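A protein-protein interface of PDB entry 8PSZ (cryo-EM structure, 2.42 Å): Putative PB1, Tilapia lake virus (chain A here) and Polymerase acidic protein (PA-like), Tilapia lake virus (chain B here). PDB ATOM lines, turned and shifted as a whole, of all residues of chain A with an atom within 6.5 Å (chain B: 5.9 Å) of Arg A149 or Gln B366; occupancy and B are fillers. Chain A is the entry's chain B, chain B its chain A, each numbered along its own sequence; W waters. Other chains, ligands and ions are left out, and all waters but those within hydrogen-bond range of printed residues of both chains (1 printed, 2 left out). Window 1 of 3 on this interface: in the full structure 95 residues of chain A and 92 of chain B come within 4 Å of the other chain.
NE2 of Gln B362 lies within hydrogen-bond range of O of Ser A15 (2.9 Å). NE2 of Gln B366 lies within hydrogen-bond range of O of Arg A149. The side-chain amide oxygen of Asn B369 is in hydrogen-bond range of the backbone NH of Cys A9, at 3.0 Å. The backbone carbonyl oxygen (O) of Leu A14 lies within hydrogen-bond range of the side-chain amide nitrogen (NE2) of Gln B362.
N of Gly A11 sits close to SG of Cys A9, 3.6 Å away. The backbone carbonyl oxygen (O) of Leu A14 is in hydrogen-bond range of the guanidinium group (NE) of Arg A149 (2.7 Å). The guanidinium group (NE) of Arg A149 lies within hydrogen-bond range of the backbone carbonyl oxygen (O) of Asn A12 (3.1 Å). The backbone carbonyl oxygen of Pro A17 sits at hydrogen-bond distance from the backbone NH of Gln A147, 2.7 Å away. A ring nitrogen (ND1) of His B367 sits at hydrogen-bond distance from the guanidinium group (NH2) of Arg B370, 3.4 Å away.
Among the printed residues, merely in contact across the chains: Gly A11 with Gln B362 (3.2 Å), Arg A149 with Gln B362 (3.4 Å), Trp A2 with Ala B365 (3.4 Å), Lys A319 with Arg B370 (3.4 Å), Lys A10 with Gln B366 (3.5 Å), Trp A2 with Val B364 (3.6 Å), Gly A150 with Gln B362 (3.6 Å), Gly A150 with Gln B366 (3.6 Å), Lys A10 with Ala B365 (3.6 Å), Gly A150 with Ala B363 (3.6 Å), Pro A17 with Gln B362 (3.9 Å), Trp A2 with Phe B368 (3.9 Å) and Trp A2 with Ser B361 (3.96 Å).
Of the printed residues of chain B, Arg A149 touches Gln B362 (3.4 Å) and Gln B366 (3.5 Å). Gln B366 touches just these residues of chain A: Lys A10 (3.5 Å), Arg A149 (3.5 Å) and Gly A150 (3.6 Å). Of the printed residues of chain A, Ala B363 touches Gly A150. Of the printed residues of chain A, Asn B369 touches Cys A9 (3.0 Å). Asn A12 touches none of the printed residues of chain B. Lys A151 touches none of the printed residues of chain B. The nearest residue of chain B that does not touch Arg A149 is Ala B363 (5.6 Å). The nearest printed residue of chain A that does not touch Ser B361 is Leu A14 (5.6 Å).
Printed residues of chain A that touch a printed residue of chain B: Trp A2, Cys A9, Lys A10, Gly A11, Leu A14, Ser A15, Pro A17, Arg A149, Gly A150 and Lys A319. Hydrophobic or aromatic side chains of chain A within 4 Å of the printed part of chain B: Trp A2, Leu A14 and Pro A17. Of the 11 printed residues of chain B, 9 touch a printed residue of chain A. Hydrophobic or aromatic side chains of chain B within 4 Å of the printed part of chain A: Ala B363, Val B364, Ala B365 and Phe B368. Among the printed residues, 17 pairs touch across the chains. Among the printed residues, no Asp or Glu carboxylate lies within 4 Å of a Lys or Arg side-chain nitrogen of the other chain.
Water W1 lies within hydrogen-bond range of O of Cys A9 (3.0 Å) and O of Ala B365 (3.1 Å).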
ATOM      1  N   TRP A   2      12.343 -11.349  28.375  1.00  0.00           N
ATOM      2  CA  TRP A   2      11.538 -12.538  28.119  1.00  0.00           C
ATOM      3  C   TRP A   2      11.560 -13.490  29.307  1.00  0.00           C
ATOM      4  O   TRP A   2      10.597 -14.234  29.524  1.00  0.00           O
ATOM      5  CB  TRP A   2      12.034 -13.253  26.860  1.00  0.00           C
ATOM      6  CG  TRP A   2      13.526 -13.414  26.805  1.00  0.00           C
ATOM      7  CD1 TRP A   2      14.409 -12.612  26.148  1.00  0.00           C
ATOM      8  CD2 TRP A   2      14.306 -14.432  27.443  1.00  0.00           C
ATOM      9  NE1 TRP A   2      15.690 -13.067  26.331  1.00  0.00           N
ATOM     10  CE2 TRP A   2      15.654 -14.183  27.123  1.00  0.00           C
ATOM     11  CE3 TRP A   2      13.996 -15.529  28.250  1.00  0.00           C
ATOM     12  CZ2 TRP A   2      16.690 -14.991  27.582  1.00  0.00           C
ATOM     13  CZ3 TRP A   2      15.026 -16.329  28.705  1.00  0.00           C
ATOM     14  CH2 TRP A   2      16.356 -16.055  28.370  1.00  0.00           C
ATOM     15  N   CYS A   9       6.117 -16.943  26.491  1.00  0.00           N
ATOM     16  CA  CYS A   9       6.797 -16.028  25.581  1.00  0.00           C
ATOM     17  C   CYS A   9       7.875 -16.794  24.833  1.00  0.00           C
ATOM     18  O   CYS A   9       8.782 -17.354  25.455  1.00  0.00           O
ATOM     19  CB  CYS A   9       7.402 -14.845  26.340  1.00  0.00           C
ATOM     20  SG  CYS A   9       8.193 -13.605  25.290  1.00  0.00           S
ATOM     21  N   LYS A  10       7.775 -16.816  23.504  1.00  0.00           N
ATOM     22  CA  LYS A  10       8.795 -17.459  22.683  1.00  0.00           C
ATOM     23  C   LYS A  10      10.054 -16.612  22.568  1.00  0.00           C
ATOM     24  O   LYS A  10      11.154 -17.161  22.438  1.00  0.00           O
ATOM     25  CB  LYS A  10       8.243 -17.747  21.285  1.00  0.00           C
ATOM     26  CG  LYS A  10       7.896 -19.198  21.035  1.00  0.00           C
ATOM     27  CD  LYS A  10       7.644 -19.459  19.557  1.00  0.00           C
ATOM     28  CE  LYS A  10       8.917 -19.850  18.830  1.00  0.00           C
ATOM     29  NZ  LYS A  10       8.641 -20.465  17.503  1.00  0.00           N
ATOM     30  N   GLY A  11       9.920 -15.290  22.612  1.00  0.00           N
ATOM     31  CA  GLY A  11      11.046 -14.404  22.403  1.00  0.00           C
ATOM     32  C   GLY A  11      11.215 -14.042  20.943  1.00  0.00           C
ATOM     33  O   GLY A  11      12.333 -14.025  20.424  1.00  0.00           O
ATOM     34  N   ASN A  12      10.104 -13.747  20.273  1.00  0.00           N
ATOM     35  CA  ASN A  12      10.090 -13.438  18.850  1.00  0.00           C
ATOM     36  C   ASN A  12      10.188 -11.945  18.565  1.00  0.00           C
ATOM     37  O   ASN A  12      10.058 -11.540  17.407  1.00  0.00           O
ATOM     38  CB  ASN A  12       8.815 -13.993  18.208  1.00  0.00           C
ATOM     39  CG  ASN A  12       8.912 -15.471  17.888  1.00  0.00           C
ATOM     40  OD1 ASN A  12       9.966 -16.086  18.038  1.00  0.00           O
ATOM     41  ND2 ASN A  12       7.805 -16.051  17.444  1.00  0.00           N
ATOM     42  N   LEU A  13      10.416 -11.118  19.586  1.00  0.00           N
ATOM     43  CA  LEU A  13      10.279  -9.677  19.404  1.00  0.00           C
ATOM     44  C   LEU A  13      11.362  -9.115  18.490  1.00  0.00           C
ATOM     45  O   LEU A  13      11.104  -8.183  17.720  1.00  0.00           O
ATOM     46  CB  LEU A  13      10.291  -8.975  20.763  1.00  0.00           C
ATOM     47  CG  LEU A  13       9.020  -9.153  21.605  1.00  0.00           C
ATOM     48  CD1 LEU A  13       9.052  -8.247  22.818  1.00  0.00           C
ATOM     49  CD2 LEU A  13       7.755  -8.899  20.793  1.00  0.00           C
ATOM     50  N   LEU A  14      12.576  -9.653  18.554  1.00  0.00           N
ATOM     51  CA  LEU A  14      13.630  -9.222  17.651  1.00  0.00           C
ATOM     52  C   LEU A  14      13.642 -10.083  16.390  1.00  0.00           C
ATOM     53  O   LEU A  14      13.019 -11.143  16.317  1.00  0.00           O
ATOM     54  CB  LEU A  14      14.991  -9.272  18.344  1.00  0.00           C
ATOM     55  CG  LEU A  14      15.208  -8.334  19.536  1.00  0.00           C
ATOM     56  CD1 LEU A  14      16.657  -8.394  19.990  1.00  0.00           C
ATOM     57  CD2 LEU A  14      14.814  -6.905  19.200  1.00  0.00           C
ATOM     58  N   SER A  15      14.370  -9.607  15.385  1.00  0.00           N
ATOM     59  CA  SER A  15      14.486 -10.325  14.126  1.00  0.00           C
ATOM     60  C   SER A  15      15.320 -11.591  14.296  1.00  0.00           C
ATOM     61  O   SER A  15      16.057 -11.763  15.272  1.00  0.00           O
ATOM     62  CB  SER A  15      15.119  -9.436  13.056  1.00  0.00           C
ATOM     63  OG  SER A  15      14.333  -8.285  12.819  1.00  0.00           O
ATOM     64  N   GLY A  16      15.195 -12.486  13.321  1.00  0.00           N
ATOM     65  CA  GLY A  16      15.951 -13.714  13.309  1.00  0.00           C
ATOM     66  C   GLY A  16      17.416 -13.473  13.007  1.00  0.00           C
ATOM     67  O   GLY A  16      17.809 -12.405  12.529  1.00  0.00           O
ATOM     68  N   PRO A  17      18.256 -14.465  13.284  1.00  0.00           N
ATOM     69  CA  PRO A  17      19.690 -14.304  13.032  1.00  0.00           C
ATOM     70  C   PRO A  17      20.000 -14.210  11.549  1.00  0.00           C
ATOM     71  O   PRO A  17      19.284 -14.746  10.701  1.00  0.00           O
ATOM     72  CB  PRO A  17      20.304 -15.566  13.646  1.00  0.00           C
ATOM     73  CG  PRO A  17      19.206 -16.562  13.658  1.00  0.00           C
ATOM     74  CD  PRO A  17      17.928 -15.800  13.813  1.00  0.00           C
ATOM     75  N   GLN A 147      17.825 -16.417   9.183  1.00  0.00           N
ATOM     76  CA  GLN A 147      16.695 -15.591   9.610  1.00  0.00           C
ATOM     77  C   GLN A 147      15.603 -16.422  10.274  1.00  0.00           C
ATOM     78  O   GLN A 147      14.430 -16.046  10.261  1.00  0.00           O
ATOM     79  CB  GLN A 147      16.113 -14.781   8.445  1.00  0.00           C
ATOM     80  CG  GLN A 147      16.855 -13.484   8.174  1.00  0.00           C
ATOM     81  CD  GLN A 147      16.500 -12.878   6.832  1.00  0.00           C
ATOM     82  OE1 GLN A 147      16.866 -13.404   5.783  1.00  0.00           O
ATOM     83  NE2 GLN A 147      15.782 -11.763   6.861  1.00  0.00           N
ATOM     84  N   GLU A 148      15.980 -17.551  10.865  1.00  0.00           N
ATOM     85  CA  GLU A 148      15.069 -18.395  11.625  1.00  0.00           C
ATOM     86  C   GLU A 148      15.391 -18.236  13.103  1.00  0.00           C
ATOM     87  O   GLU A 148      16.496 -18.573  13.539  1.00  0.00           O
ATOM     88  CB  GLU A 148      15.193 -19.857  11.199  1.00  0.00           C
ATOM     89  CG  GLU A 148      14.842 -20.105   9.745  1.00  0.00           C
ATOM     90  CD  GLU A 148      14.444 -21.541   9.482  1.00  0.00           C
ATOM     91  OE1 GLU A 148      13.253 -21.868   9.665  1.00  0.00           O
ATOM     92  OE2 GLU A 148      15.320 -22.343   9.098  1.00  0.00           O
ATOM     93  N   ARG A 149      14.429 -17.727  13.866  1.00  0.00           N
ATOM     94  CA  ARG A 149      14.665 -17.443  15.274  1.00  0.00           C
ATOM     95  C   ARG A 149      15.006 -18.720  16.031  1.00  0.00           C
ATOM     96  O   ARG A 149      14.414 -19.776  15.801  1.00  0.00           O
ATOM     97  CB  ARG A 149      13.433 -16.782  15.890  1.00  0.00           C
ATOM     98  CG  ARG A 149      13.048 -15.472  15.236  1.00  0.00           C
ATOM     99  CD  ARG A 149      12.170 -14.640  16.148  1.00  0.00           C
ATOM    100  NE  ARG A 149      11.786 -13.374  15.537  1.00  0.00           N
ATOM    101  CZ  ARG A 149      10.753 -13.211  14.722  1.00  0.00           C
ATOM    102  NH1 ARG A 149       9.961 -14.218  14.396  1.00  0.00           N
ATOM    103  NH2 ARG A 149      10.507 -12.004  14.222  1.00  0.00           N
ATOM    104  N   GLY A 150      15.969 -18.615  16.943  1.00  0.00           N
ATOM    105  CA  GLY A 150      16.370 -19.745  17.754  1.00  0.00           C
ATOM    106  C   GLY A 150      17.361 -20.681  17.108  1.00  0.00           C
ATOM    107  O   GLY A 150      17.656 -21.735  17.683  1.00  0.00           O
ATOM    108  N   LYS A 151      17.891 -20.334  15.936  1.00  0.00           N
ATOM    109  CA  LYS A 151      18.866 -21.158  15.222  1.00  0.00           C
ATOM    110  C   LYS A 151      20.071 -20.291  14.883  1.00  0.00           C
ATOM    111  O   LYS A 151      20.211 -19.820  13.747  1.00  0.00           O
ATOM    112  CB  LYS A 151      18.257 -21.768  13.959  1.00  0.00           C
ATOM    113  CG  LYS A 151      17.210 -22.836  14.228  1.00  0.00           C
ATOM    114  CD  LYS A 151      17.079 -23.793  13.057  1.00  0.00           C
ATOM    115  CE  LYS A 151      18.227 -24.790  13.010  1.00  0.00           C
ATOM    116  NZ  LYS A 151      17.805 -26.152  13.435  1.00  0.00           N
ATOM    117  N   PRO A 152      20.968 -20.062  15.846  1.00  0.00           N
ATOM    118  CA  PRO A 152      22.159 -19.252  15.547  1.00  0.00           C
ATOM    119  C   PRO A 152      22.988 -19.820  14.413  1.00  0.00           C
ATOM    120  O   PRO A 152      23.604 -19.057  13.659  1.00  0.00           O
ATOM    121  CB  PRO A 152      22.932 -19.252  16.874  1.00  0.00           C
ATOM    122  CG  PRO A 152      21.945 -19.666  17.910  1.00  0.00           C
ATOM    123  CD  PRO A 152      20.965 -20.557  17.232  1.00  0.00           C
ATOM    124  N   LYS A 319      14.070 -31.347  24.024  1.00  0.00           N
ATOM    125  CA  LYS A 319      12.956 -30.408  23.953  1.00  0.00           C
ATOM    126  C   LYS A 319      11.607 -31.002  24.324  1.00  0.00           C
ATOM    127  O   LYS A 319      10.720 -30.254  24.740  1.00  0.00           O
ATOM    128  CB  LYS A 319      12.858 -29.818  22.540  1.00  0.00           C
ATOM    129  CG  LYS A 319      14.153 -29.203  22.052  1.00  0.00           C
ATOM    130  CD  LYS A 319      13.940 -28.338  20.825  1.00  0.00           C
ATOM    131  CE  LYS A 319      15.211 -27.597  20.450  1.00  0.00           C
ATOM    132  NZ  LYS A 319      14.985 -26.597  19.373  1.00  0.00           N
ATOM    133  N   CYS A 346       3.765 -16.130  20.521  1.00  0.00           N
ATOM    134  CA  CYS A 346       4.586 -16.038  19.321  1.00  0.00           C
ATOM    135  C   CYS A 346       4.628 -14.633  18.737  1.00  0.00           C
ATOM    136  O   CYS A 346       5.137 -14.454  17.626  1.00  0.00           O
ATOM    137  CB  CYS A 346       4.074 -17.016  18.260  1.00  0.00           C
ATOM    138  SG  CYS A 346       4.183 -18.747  18.737  1.00  0.00           S
ATOM    139  N   THR A 347       4.108 -13.638  19.453  1.00  0.00           N
ATOM    140  CA  THR A 347       4.072 -12.278  18.932  1.00  0.00           C
ATOM    141  C   THR A 347       5.470 -11.824  18.532  1.00  0.00           C
ATOM    142  O   THR A 347       6.427 -11.964  19.298  1.00  0.00           O
ATOM    143  CB  THR A 347       3.490 -11.327  19.978  1.00  0.00           C
ATOM    144  OG1 THR A 347       2.232 -11.835  20.441  1.00  0.00           O
ATOM    145  CG2 THR A 347       3.290  -9.941  19.391  1.00  0.00           C
ATOM    146  N   ALA A 348       5.579 -11.269  17.329  1.00  0.00           N
ATOM    147  CA  ALA A 348       6.854 -10.862  16.761  1.00  0.00           C
ATOM    148  C   ALA A 348       6.882  -9.352  16.582  1.00  0.00           C
ATOM    149  O   ALA A 348       5.857  -8.733  16.281  1.00  0.00           O
ATOM    150  CB  ALA A 348       7.102 -11.552  15.415  1.00  0.00           C
ATOM    151  N   GLY A 349       8.060  -8.763  16.778  1.00  0.00           N
ATOM    152  CA  GLY A 349       8.230  -7.344  16.571  1.00  0.00           C
ATOM    153  C   GLY A 349       8.354  -6.990  15.102  1.00  0.00           C
ATOM    154  O   GLY A 349       8.581  -7.837  14.242  1.00  0.00           O
ATOM    155  N   SER B 361      20.007 -15.435  22.319  1.00  0.00           N
ATOM    156  CA  SER B 361      19.013 -15.236  23.363  1.00  0.00           C
ATOM    157  C   SER B 361      17.650 -15.768  22.942  1.00  0.00           C
ATOM    158  O   SER B 361      16.846 -16.138  23.797  1.00  0.00           O
ATOM    159  CB  SER B 361      18.919 -13.753  23.724  1.00  0.00           C
ATOM    160  OG  SER B 361      18.380 -12.997  22.657  1.00  0.00           O
ATOM    161  N   GLN B 362      17.375 -15.834  21.637  1.00  0.00           N
ATOM    162  CA  GLN B 362      16.111 -16.410  21.183  1.00  0.00           C
ATOM    163  C   GLN B 362      16.046 -17.905  21.474  1.00  0.00           C
ATOM    164  O   GLN B 362      15.013 -18.413  21.927  1.00  0.00           O
ATOM    165  CB  GLN B 362      15.919 -16.146  19.691  1.00  0.00           C
ATOM    166  CG  GLN B 362      15.309 -14.794  19.386  1.00  0.00           C
ATOM    167  CD  GLN B 362      15.621 -14.307  17.989  1.00  0.00           C
ATOM    168  OE1 GLN B 362      16.127 -15.055  17.154  1.00  0.00           O
ATOM    169  NE2 GLN B 362      15.321 -13.044  17.725  1.00  0.00           N
ATOM    170  N   ALA B 363      17.140 -18.628  21.221  1.00  0.00           N
ATOM    171  CA  ALA B 363      17.183 -20.044  21.567  1.00  0.00           C
ATOM    172  C   ALA B 363      17.057 -20.240  23.071  1.00  0.00           C
ATOM    173  O   ALA B 363      16.320 -21.126  23.536  1.00  0.00           O
ATOM    174  CB  ALA B 363      18.477 -20.670  21.049  1.00  0.00           C
ATOM    175  N   VAL B 364      17.755 -19.412  23.851  1.00  0.00           N
ATOM    176  CA  VAL B 364      17.647 -19.523  25.304  1.00  0.00           C
ATOM    177  C   VAL B 364      16.213 -19.254  25.752  1.00  0.00           C
ATOM    178  O   VAL B 364      15.686 -19.939  26.633  1.00  0.00           O
ATOM    179  CB  VAL B 364      18.645 -18.576  25.997  1.00  0.00           C
ATOM    180  CG1 VAL B 364      18.550 -18.714  27.510  1.00  0.00           C
ATOM    181  CG2 VAL B 364      20.063 -18.862  25.536  1.00  0.00           C
ATOM    182  N   ALA B 365      15.563 -18.251  25.157  1.00  0.00           N
ATOM    183  CA  ALA B 365      14.195 -17.910  25.531  1.00  0.00           C
ATOM    184  C   ALA B 365      13.223 -19.031  25.187  1.00  0.00           C
ATOM    185  O   ALA B 365      12.315 -19.329  25.969  1.00  0.00           O
ATOM    186  CB  ALA B 365      13.773 -16.614  24.841  1.00  0.00           C
ATOM    187  N   GLN B 366      13.385 -19.654  24.018  1.00  0.00           N
ATOM    188  CA  GLN B 366      12.514 -20.769  23.660  1.00  0.00           C
ATOM    189  C   GLN B 366      12.686 -21.931  24.630  1.00  0.00           C
ATOM    190  O   GLN B 366      11.698 -22.519  25.103  1.00  0.00           O
ATOM    191  CB  GLN B 366      12.804 -21.215  22.227  1.00  0.00           C
ATOM    192  CG  GLN B 366      12.321 -20.236  21.172  1.00  0.00           C
ATOM    193  CD  GLN B 366      12.858 -20.547  19.791  1.00  0.00           C
ATOM    194  OE1 GLN B 366      13.128 -21.701  19.462  1.00  0.00           O
ATOM    195  NE2 GLN B 366      13.017 -19.516  18.973  1.00  0.00           N
ATOM    196  N   HIS B 367      13.936 -22.268  24.958  1.00  0.00           N
ATOM    197  CA  HIS B 367      14.159 -23.366  25.890  1.00  0.00           C
ATOM    198  C   HIS B 367      13.612 -23.034  27.273  1.00  0.00           C
ATOM    199  O   HIS B 367      13.063 -23.905  27.956  1.00  0.00           O
ATOM    200  CB  HIS B 367      15.644 -23.712  25.963  1.00  0.00           C
ATOM    201  CG  HIS B 367      15.913 -25.043  26.590  1.00  0.00           C
ATOM    202  ND1 HIS B 367      15.326 -26.206  26.142  1.00  0.00           N
ATOM    203  CD2 HIS B 367      16.687 -25.395  27.642  1.00  0.00           C
ATOM    204  CE1 HIS B 367      15.735 -27.218  26.885  1.00  0.00           C
ATOM    205  NE2 HIS B 367      16.562 -26.752  27.802  1.00  0.00           N
ATOM    206  N   PHE B 368      13.741 -21.775  27.704  1.00  0.00           N
ATOM    207  CA  PHE B 368      13.214 -21.389  29.010  1.00  0.00           C
ATOM    208  C   PHE B 368      11.691 -21.379  29.026  1.00  0.00           C
ATOM    209  O   PHE B 368      11.083 -21.665  30.061  1.00  0.00           O
ATOM    210  CB  PHE B 368      13.753 -20.017  29.413  1.00  0.00           C
ATOM    211  CG  PHE B 368      13.417 -19.625  30.824  1.00  0.00           C
ATOM    212  CD1 PHE B 368      13.715 -20.466  31.881  1.00  0.00           C
ATOM    213  CD2 PHE B 368      12.803 -18.416  31.094  1.00  0.00           C
ATOM    214  CE1 PHE B 368      13.408 -20.109  33.176  1.00  0.00           C
ATOM    215  CE2 PHE B 368      12.495 -18.055  32.388  1.00  0.00           C
ATOM    216  CZ  PHE B 368      12.797 -18.902  33.430  1.00  0.00           C
ATOM    217  N   ASN B 369      11.058 -21.037  27.902  1.00  0.00           N
ATOM    218  CA  ASN B 369       9.607 -21.157  27.804  1.00  0.00           C
ATOM    219  C   ASN B 369       9.182 -22.606  27.995  1.00  0.00           C
ATOM    220  O   ASN B 369       8.270 -22.907  28.782  1.00  0.00           O
ATOM    221  CB  ASN B 369       9.141 -20.625  26.449  1.00  0.00           C
ATOM    222  CG  ASN B 369       7.666 -20.284  26.428  1.00  0.00           C
ATOM    223  OD1 ASN B 369       7.151 -19.635  27.336  1.00  0.00           O
ATOM    224  ND2 ASN B 369       6.978 -20.718  25.382  1.00  0.00           N
ATOM    225  N   ARG B 370       9.862 -23.526  27.307  1.00  0.00           N
ATOM    226  CA  ARG B 370       9.586 -24.944  27.520  1.00  0.00           C
ATOM    227  C   ARG B 370       9.796 -25.327  28.980  1.00  0.00           C
ATOM    228  O   ARG B 370       8.994 -26.066  29.560  1.00  0.00           O
ATOM    229  CB  ARG B 370      10.474 -25.799  26.619  1.00  0.00           C
ATOM    230  CG  ARG B 370      10.069 -25.792  25.164  1.00  0.00           C
ATOM    231  CD  ARG B 370      10.851 -26.827  24.379  1.00  0.00           C
ATOM    232  NE  ARG B 370      12.239 -26.433  24.176  1.00  0.00           N
ATOM    233  CZ  ARG B 370      12.668 -25.660  23.187  1.00  0.00           C
ATOM    234  NH1 ARG B 370      11.838 -25.168  22.282  1.00  0.00           N
ATOM    235  NH2 ARG B 370      13.964 -25.378  23.102  1.00  0.00           N
ATOM    236  N   HIS B 371      10.873 -24.825  29.588  1.00  0.00           N
ATOM    237  CA  HIS B 371      11.168 -25.131  30.984  1.00  0.00           C
ATOM    238  C   HIS B 371      10.026 -24.689  31.891  1.00  0.00           C
ATOM    239  O   HIS B 371       9.565 -25.451  32.748  1.00  0.00           O
ATOM    240  CB  HIS B 371      12.481 -24.446  31.380  1.00  0.00           C
ATOM    241  CG  HIS B 371      12.910 -24.693  32.795  1.00  0.00           C
ATOM    242  ND1 HIS B 371      14.098 -24.210  33.299  1.00  0.00           N
ATOM    243  CD2 HIS B 371      12.324 -25.375  33.805  1.00  0.00           C
ATOM    244  CE1 HIS B 371      14.220 -24.577  34.562  1.00  0.00           C
ATOM    245  NE2 HIS B 371      13.157 -25.285  34.893  1.00  0.00           N
HETATM  246  O   HOH W   1      10.767 -17.269  27.767  1.00  0.00           O
